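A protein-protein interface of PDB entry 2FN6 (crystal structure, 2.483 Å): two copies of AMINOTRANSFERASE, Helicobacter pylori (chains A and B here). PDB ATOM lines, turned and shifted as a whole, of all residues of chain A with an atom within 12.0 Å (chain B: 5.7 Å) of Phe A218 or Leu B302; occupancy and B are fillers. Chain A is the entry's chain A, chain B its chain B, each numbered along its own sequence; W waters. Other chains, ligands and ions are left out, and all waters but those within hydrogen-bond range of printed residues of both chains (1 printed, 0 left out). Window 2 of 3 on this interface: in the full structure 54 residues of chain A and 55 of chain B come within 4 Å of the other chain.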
ATOM      1  N   MET A 212       4.092  -4.200  13.380  1.00  0.00           N
ATOM      2  CA  MET A 212       5.160  -3.214  13.493  1.00  0.00           C
ATOM      3  C   MET A 212       5.326  -2.387  12.216  1.00  0.00           C
ATOM      4  O   MET A 212       5.597  -2.934  11.144  1.00  0.00           O
ATOM      5  CB  MET A 212       6.473  -3.906  13.864  1.00  0.00           C
ATOM      6  CG  MET A 212       7.676  -2.968  14.021  1.00  0.00           C
ATOM      7  SD  MET A 212       7.647  -1.943  15.513  1.00  0.00           S
ATOM      8  CE  MET A 212       7.640  -3.190  16.806  1.00  0.00           C
ATOM      9  N   LEU A 213       5.147  -1.069  12.343  1.00  0.00           N
ATOM     10  CA  LEU A 213       5.381  -0.127  11.239  1.00  0.00           C
ATOM     11  C   LEU A 213       6.722   0.544  11.452  1.00  0.00           C
ATOM     12  O   LEU A 213       7.039   0.940  12.563  1.00  0.00           O
ATOM     13  CB  LEU A 213       4.276   0.932  11.147  1.00  0.00           C
ATOM     14  CG  LEU A 213       2.834   0.441  10.988  1.00  0.00           C
ATOM     15  CD1 LEU A 213       2.056   0.638  12.277  1.00  0.00           C
ATOM     16  CD2 LEU A 213       2.126   1.150   9.832  1.00  0.00           C
ATOM     17  N   LYS A 214       7.513   0.657  10.394  1.00  0.00           N
ATOM     18  CA  LYS A 214       8.826   1.297  10.507  1.00  0.00           C
ATOM     19  C   LYS A 214       8.662   2.774  10.878  1.00  0.00           C
ATOM     20  O   LYS A 214       7.656   3.400  10.536  1.00  0.00           O
ATOM     21  CB  LYS A 214       9.637   1.144   9.210  1.00  0.00           C
ATOM     22  N   LYS A 215       9.632   3.302  11.621  1.00  0.00           N
ATOM     23  CA  LYS A 215       9.704   4.735  11.941  1.00  0.00           C
ATOM     24  C   LYS A 215      11.175   5.173  12.101  1.00  0.00           C
ATOM     25  O   LYS A 215      11.970   5.033  11.164  1.00  0.00           O
ATOM     26  CB  LYS A 215       8.841   5.088  13.165  1.00  0.00           C
ATOM     27  N   ASP A 216      11.543   5.663  13.285  1.00  0.00           N
ATOM     28  CA  ASP A 216      12.879   6.225  13.537  1.00  0.00           C
ATOM     29  C   ASP A 216      14.088   5.507  12.899  1.00  0.00           C
ATOM     30  O   ASP A 216      15.039   6.173  12.490  1.00  0.00           O
ATOM     31  CB  ASP A 216      13.107   6.389  15.044  1.00  0.00           C
ATOM     32  N   PHE A 217      14.032   4.176  12.792  1.00  0.00           N
ATOM     33  CA  PHE A 217      15.199   3.307  12.520  1.00  0.00           C
ATOM     34  C   PHE A 217      15.494   2.552  13.812  1.00  0.00           C
ATOM     35  O   PHE A 217      15.972   1.417  13.788  1.00  0.00           O
ATOM     36  CB  PHE A 217      16.444   4.104  12.083  1.00  0.00           C
ATOM     37  CG  PHE A 217      17.572   3.256  11.521  1.00  0.00           C
ATOM     38  CD1 PHE A 217      17.954   3.389  10.181  1.00  0.00           C
ATOM     39  CD2 PHE A 217      18.270   2.346  12.330  1.00  0.00           C
ATOM     40  CE1 PHE A 217      19.003   2.618   9.650  1.00  0.00           C
ATOM     41  CE2 PHE A 217      19.310   1.565  11.810  1.00  0.00           C
ATOM     42  CZ  PHE A 217      19.680   1.702  10.469  1.00  0.00           C
ATOM     43  N   PHE A 218      15.210   3.205  14.940  1.00  0.00           N
ATOM     44  CA  PHE A 218      15.332   2.607  16.270  1.00  0.00           C
ATOM     45  C   PHE A 218      13.954   2.370  16.877  1.00  0.00           C
ATOM     46  O   PHE A 218      13.769   1.470  17.701  1.00  0.00           O
ATOM     47  CB  PHE A 218      16.126   3.517  17.210  1.00  0.00           C
ATOM     48  CG  PHE A 218      17.421   4.004  16.639  1.00  0.00           C
ATOM     49  CD1 PHE A 218      17.477   5.206  15.940  1.00  0.00           C
ATOM     50  CD2 PHE A 218      18.585   3.268  16.806  1.00  0.00           C
ATOM     51  CE1 PHE A 218      18.675   5.665  15.409  1.00  0.00           C
ATOM     52  CE2 PHE A 218      19.790   3.718  16.283  1.00  0.00           C
ATOM     53  CZ  PHE A 218      19.837   4.917  15.580  1.00  0.00           C
ATOM     54  N   GLU A 219      12.996   3.194  16.465  1.00  0.00           N
ATOM     55  CA  GLU A 219      11.655   3.167  17.019  1.00  0.00           C
ATOM     56  C   GLU A 219      10.649   2.732  15.959  1.00  0.00           C
ATOM     57  O   GLU A 219      10.775   3.078  14.784  1.00  0.00           O
ATOM     58  CB  GLU A 219      11.293   4.555  17.553  1.00  0.00           C
ATOM     59  CG  GLU A 219      10.026   4.621  18.406  1.00  0.00           C
ATOM     60  CD  GLU A 219       9.618   6.053  18.745  1.00  0.00           C
ATOM     61  OE1 GLU A 219       8.459   6.272  19.164  1.00  0.00           O
ATOM     62  OE2 GLU A 219      10.461   6.964  18.591  1.00  0.00           O
ATOM     63  N   GLY A 220       9.655   1.962  16.384  1.00  0.00           N
ATOM     64  CA  GLY A 220       8.560   1.580  15.508  1.00  0.00           C
ATOM     65  C   GLY A 220       7.229   1.964  16.115  1.00  0.00           C
ATOM     66  O   GLY A 220       7.177   2.462  17.240  1.00  0.00           O
ATOM     67  N   GLU A 221       6.155   1.731  15.366  1.00  0.00           N
ATOM     68  CA  GLU A 221       4.798   1.981  15.853  1.00  0.00           C
ATOM     69  C   GLU A 221       3.925   0.741  15.702  1.00  0.00           C
ATOM     70  O   GLU A 221       4.059   0.004  14.724  1.00  0.00           O
ATOM     71  CB  GLU A 221       4.162   3.182  15.123  1.00  0.00           C
ATOM     72  CG  GLU A 221       2.842   3.684  15.742  1.00  0.00           C
ATOM     73  CD  GLU A 221       2.900   3.792  17.270  1.00  0.00           C
ATOM     74  OE1 GLU A 221       3.726   4.561  17.794  1.00  0.00           O
ATOM     75  OE2 GLU A 221       2.126   3.099  17.955  1.00  0.00           O
ATOM     76  N   VAL A 222       3.041   0.525  16.676  1.00  0.00           N
ATOM     77  CA  VAL A 222       2.085  -0.582  16.661  1.00  0.00           C
ATOM     78  C   VAL A 222       0.656  -0.056  16.864  1.00  0.00           C
ATOM     79  O   VAL A 222       0.315   0.438  17.947  1.00  0.00           O
ATOM     80  CB  VAL A 222       2.421  -1.665  17.747  1.00  0.00           C
ATOM     81  CG1 VAL A 222       1.457  -2.835  17.655  1.00  0.00           C
ATOM     82  CG2 VAL A 222       3.845  -2.168  17.610  1.00  0.00           C
ATOM     83  N   CYS B 297      20.098  13.844  24.161  1.00  0.00           N
ATOM     84  CA  CYS B 297      20.735  13.820  22.839  1.00  0.00           C
ATOM     85  C   CYS B 297      20.834  12.434  22.180  1.00  0.00           C
ATOM     86  O   CYS B 297      21.473  12.289  21.131  1.00  0.00           O
ATOM     87  CB  CYS B 297      22.107  14.510  22.895  1.00  0.00           C
ATOM     88  SG  CYS B 297      23.096  14.124  24.365  1.00  0.00           S
ATOM     89  N   LYS B 298      20.181  11.435  22.782  1.00  0.00           N
ATOM     90  CA  LYS B 298      20.148  10.063  22.259  1.00  0.00           C
ATOM     91  C   LYS B 298      20.164   9.973  20.734  1.00  0.00           C
ATOM     92  O   LYS B 298      20.987   9.262  20.167  1.00  0.00           O
ATOM     93  CB  LYS B 298      18.943   9.296  22.814  1.00  0.00           C
ATOM     94  CG  LYS B 298      19.278   8.309  23.928  1.00  0.00           C
ATOM     95  CD  LYS B 298      19.509   6.903  23.385  1.00  0.00           C
ATOM     96  CE  LYS B 298      18.261   6.037  23.493  1.00  0.00           C
ATOM     97  NZ  LYS B 298      18.210   5.299  24.787  1.00  0.00           N
ATOM     98  N   LYS B 299      19.265  10.700  20.077  1.00  0.00           N
ATOM     99  CA  LYS B 299      19.173  10.678  18.621  1.00  0.00           C
ATOM    100  C   LYS B 299      20.518  10.924  17.941  1.00  0.00           C
ATOM    101  O   LYS B 299      20.871  10.222  16.985  1.00  0.00           O
ATOM    102  CB  LYS B 299      18.145  11.697  18.123  1.00  0.00           C
ATOM    103  CG  LYS B 299      16.700  11.220  18.152  1.00  0.00           C
ATOM    104  CD  LYS B 299      16.306  10.510  16.854  1.00  0.00           C
ATOM    105  CE  LYS B 299      14.789  10.483  16.672  1.00  0.00           C
ATOM    106  NZ  LYS B 299      14.347   9.361  15.795  1.00  0.00           N
ATOM    107  N   LEU B 300      21.268  11.909  18.435  1.00  0.00           N
ATOM    108  CA  LEU B 300      22.549  12.287  17.823  1.00  0.00           C
ATOM    109  C   LEU B 300      23.713  11.374  18.205  1.00  0.00           C
ATOM    110  O   LEU B 300      24.643  11.185  17.410  1.00  0.00           O
ATOM    111  CB  LEU B 300      22.892  13.759  18.112  1.00  0.00           C
ATOM    112  CG  LEU B 300      22.387  14.756  17.060  1.00  0.00           C
ATOM    113  CD1 LEU B 300      22.269  16.158  17.640  1.00  0.00           C
ATOM    114  CD2 LEU B 300      23.274  14.746  15.801  1.00  0.00           C
ATOM    115  N   ILE B 301      23.657  10.823  19.418  1.00  0.00           N
ATOM    116  CA  ILE B 301      24.668   9.879  19.911  1.00  0.00           C
ATOM    117  C   ILE B 301      24.598   8.538  19.144  1.00  0.00           C
ATOM    118  O   ILE B 301      25.633   7.953  18.790  1.00  0.00           O
ATOM    119  CB  ILE B 301      24.550   9.661  21.449  1.00  0.00           C
ATOM    120  CG1 ILE B 301      24.733  10.994  22.191  1.00  0.00           C
ATOM    121  CG2 ILE B 301      25.553   8.612  21.934  1.00  0.00           C
ATOM    122  CD1 ILE B 301      24.942  10.887  23.691  1.00  0.00           C
ATOM    123  N   LEU B 302      23.376   8.077  18.873  1.00  0.00           N
ATOM    124  CA  LEU B 302      23.164   6.838  18.141  1.00  0.00           C
ATOM    125  C   LEU B 302      23.542   6.970  16.662  1.00  0.00           C
ATOM    126  O   LEU B 302      24.147   6.055  16.093  1.00  0.00           O
ATOM    127  CB  LEU B 302      21.716   6.360  18.289  1.00  0.00           C
ATOM    128  CG  LEU B 302      21.233   5.893  19.666  1.00  0.00           C
ATOM    129  CD1 LEU B 302      19.723   5.694  19.652  1.00  0.00           C
ATOM    130  CD2 LEU B 302      21.933   4.619  20.105  1.00  0.00           C
ATOM    131  N   GLU B 303      23.201   8.106  16.048  1.00  0.00           N
ATOM    132  CA  GLU B 303      23.543   8.351  14.642  1.00  0.00           C
ATOM    133  C   GLU B 303      25.048   8.419  14.410  1.00  0.00           C
ATOM    134  O   GLU B 303      25.534   8.009  13.351  1.00  0.00           O
ATOM    135  CB  GLU B 303      22.858   9.606  14.114  1.00  0.00           C
ATOM    136  CG  GLU B 303      21.430   9.341  13.638  1.00  0.00           C
ATOM    137  CD  GLU B 303      20.534  10.576  13.688  1.00  0.00           C
ATOM    138  OE1 GLU B 303      21.062  11.711  13.738  1.00  0.00           O
ATOM    139  OE2 GLU B 303      19.293  10.408  13.676  1.00  0.00           O
ATOM    140  N   SER B 304      25.782   8.915  15.402  1.00  0.00           N
ATOM    141  CA  SER B 304      27.239   8.942  15.306  1.00  0.00           C
ATOM    142  C   SER B 304      27.875   7.585  15.668  1.00  0.00           C
ATOM    143  O   SER B 304      28.994   7.295  15.249  1.00  0.00           O
ATOM    144  CB  SER B 304      27.845  10.116  16.091  1.00  0.00           C
ATOM    145  OG  SER B 304      28.074   9.801  17.449  1.00  0.00           O
ATOM    146  N   LEU B 305      27.162   6.752  16.427  1.00  0.00           N
ATOM    147  CA  LEU B 305      27.593   5.370  16.624  1.00  0.00           C
ATOM    148  C   LEU B 305      27.434   4.615  15.313  1.00  0.00           C
ATOM    149  O   LEU B 305      28.371   3.970  14.864  1.00  0.00           O
ATOM    150  CB  LEU B 305      26.826   4.685  17.752  1.00  0.00           C
ATOM    151  CG  LEU B 305      27.195   5.104  19.174  1.00  0.00           C
ATOM    152  CD1 LEU B 305      26.183   4.548  20.158  1.00  0.00           C
ATOM    153  CD2 LEU B 305      28.611   4.680  19.559  1.00  0.00           C
ATOM    154  N   HIS B 306      26.256   4.722  14.697  1.00  0.00           N
ATOM    155  CA  HIS B 306      25.991   4.172  13.364  1.00  0.00           C
ATOM    156  C   HIS B 306      26.980   4.723  12.328  1.00  0.00           C
ATOM    157  O   HIS B 306      27.396   4.006  11.398  1.00  0.00           O
ATOM    158  CB  HIS B 306      24.550   4.496  12.918  1.00  0.00           C
ATOM    159  CG  HIS B 306      24.148   3.874  11.608  1.00  0.00           C
ATOM    160  ND1 HIS B 306      23.017   3.097  11.470  1.00  0.00           N
ATOM    161  CD2 HIS B 306      24.713   3.928  10.377  1.00  0.00           C
ATOM    162  CE1 HIS B 306      22.906   2.696  10.217  1.00  0.00           C
ATOM    163  NE2 HIS B 306      23.926   3.181   9.533  1.00  0.00           N
ATOM    164  N   LYS B 307      27.362   5.989  12.505  1.00  0.00           N
ATOM    165  CA  LYS B 307      28.282   6.654  11.591  1.00  0.00           C
ATOM    166  C   LYS B 307      29.624   5.922  11.585  1.00  0.00           C
ATOM    167  O   LYS B 307      30.210   5.698  10.524  1.00  0.00           O
ATOM    168  CB  LYS B 307      28.456   8.123  11.986  1.00  0.00           C
ATOM    169  CG  LYS B 307      28.675   9.107  10.824  1.00  0.00           C
ATOM    170  CD  LYS B 307      28.512  10.563  11.301  1.00  0.00           C
ATOM    171  CE  LYS B 307      29.133  11.571  10.332  1.00  0.00           C
ATOM    172  NZ  LYS B 307      28.407  11.655   9.031  1.00  0.00           N
ATOM    173  N   ILE B 310      28.988   1.094  14.155  1.00  0.00           N
ATOM    174  CA  ILE B 310      28.377   0.371  15.261  1.00  0.00           C
ATOM    175  C   ILE B 310      26.847   0.488  15.162  1.00  0.00           C
ATOM    176  O   ILE B 310      26.279   1.527  15.498  1.00  0.00           O
ATOM    177  CB  ILE B 310      28.900   0.946  16.597  1.00  0.00           C
ATOM    178  CG1 ILE B 310      30.433   0.879  16.620  1.00  0.00           C
ATOM    179  CG2 ILE B 310      28.300   0.224  17.804  1.00  0.00           C
ATOM    180  CD1 ILE B 310      31.080   1.899  17.510  1.00  0.00           C
ATOM    181  N   ALA B 312      24.212   0.082  16.800  1.00  0.00           N
ATOM    182  CA  ALA B 312      23.617  -0.070  18.121  1.00  0.00           C
ATOM    183  C   ALA B 312      22.088   0.026  18.055  1.00  0.00           C
ATOM    184  O   ALA B 312      21.524   0.524  17.070  1.00  0.00           O
ATOM    185  CB  ALA B 312      24.184   0.963  19.063  1.00  0.00           C
ATOM    186  N   GLN B 313      21.434  -0.486  19.096  1.00  0.00           N
ATOM    187  CA  GLN B 313      19.971  -0.580  19.155  1.00  0.00           C
ATOM    188  C   GLN B 313      19.500  -0.313  20.571  1.00  0.00           C
ATOM    189  O   GLN B 313      20.308  -0.322  21.507  1.00  0.00           O
ATOM    190  CB  GLN B 313      19.495  -1.963  18.716  1.00  0.00           C
ATOM    191  CG  GLN B 313      19.537  -2.190  17.214  1.00  0.00           C
ATOM    192  CD  GLN B 313      18.449  -1.426  16.490  1.00  0.00           C
ATOM    193  OE1 GLN B 313      17.263  -1.624  16.756  1.00  0.00           O
ATOM    194  NE2 GLN B 313      18.846  -0.539  15.570  1.00  0.00           N
ATOM    195  N   VAL B 314      18.202  -0.072  20.729  1.00  0.00           N
ATOM    196  CA  VAL B 314      17.630   0.201  22.045  1.00  0.00           C
ATOM    197  C   VAL B 314      16.570  -0.846  22.345  1.00  0.00           C
ATOM    198  O   VAL B 314      15.664  -1.067  21.535  1.00  0.00           O
ATOM    199  CB  VAL B 314      16.982   1.630  22.126  1.00  0.00           C
ATOM    200  CG1 VAL B 314      16.388   1.883  23.508  1.00  0.00           C
ATOM    201  CG2 VAL B 314      17.996   2.726  21.797  1.00  0.00           C
ATOM    202  N   ILE B 345      21.284   1.720  25.621  1.00  0.00           N
ATOM    203  CA  ILE B 345      21.779   1.385  24.293  1.00  0.00           C
ATOM    204  C   ILE B 345      22.373  -0.021  24.392  1.00  0.00           C
ATOM    205  O   ILE B 345      23.093  -0.328  25.351  1.00  0.00           O
ATOM    206  CB  ILE B 345      22.872   2.371  23.819  1.00  0.00           C
ATOM    207  CG1 ILE B 345      22.354   3.808  23.827  1.00  0.00           C
ATOM    208  CG2 ILE B 345      23.394   1.996  22.423  1.00  0.00           C
ATOM    209  CD1 ILE B 345      23.453   4.821  23.836  1.00  0.00           C
HETATM  210  O   HOH W   1      16.881   0.628  18.723  1.00  0.00           O
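Among the printed residues, pairs that only touch across the chains: Asp A216 with Lys B299 (3.3 Å), Phe A217 with His B306 (3.4 Å), Phe A218 with Leu B302 (3.6 Å), Phe A218 with Ala B312 (3.7 Å) and Phe A217 with Gln B313 (3.9 Å).
Met A212 touches none of the printed residues of chain B. Lys A215 touches none of the printed residues of chain B. Of the printed residues of chain B, Asp A216 touches Lys B299 (3.3 Å). Printed residues of chain B within 4 Å of Phe A217: His B306 and Gln B313. Of the printed residues of chain B, Phe A218 touches Leu B302 (3.6 Å) and Ala B312 (3.7 Å). No residue of chain A comes within 4 Å of Lys B298. No residue of chain A comes within 4 Å of Ile B301. No residue of chain A comes within 4 Å of Glu B303. No residue of chain A comes within 4 Å of Ser B304. Of the printed residues of chain A, His B306 touches Phe A217 (3.4 Å). Ala B312 touches just one residue of chain A: Phe A218 (3.7 Å). Of the printed residues of chain A, Gln B313 touches Phe A217. No residue of chain A comes within 4 Å of Ile B345.
Printed residues of chain A that touch a printed residue of chain B: Asp A216, Phe A217 and Phe A218. Hydrophobic or aromatic side chains of chain A that line the printed part of chain B: Phe A217 and Phe A218. Among the printed residues, 5 pairs touch across the chains. Among the printed residues, no Asp or Glu carboxylate lies within 4 Å of a Lys or Arg side-chain nitrogen of the other chain.
No position is printed for both chains.
Water W1 lies within hydrogen-bond range of N of Val B314 (2.5 Å), OE1 of Gln B313 (3.0 Å) and O of Phe A218 (3.4 Å).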
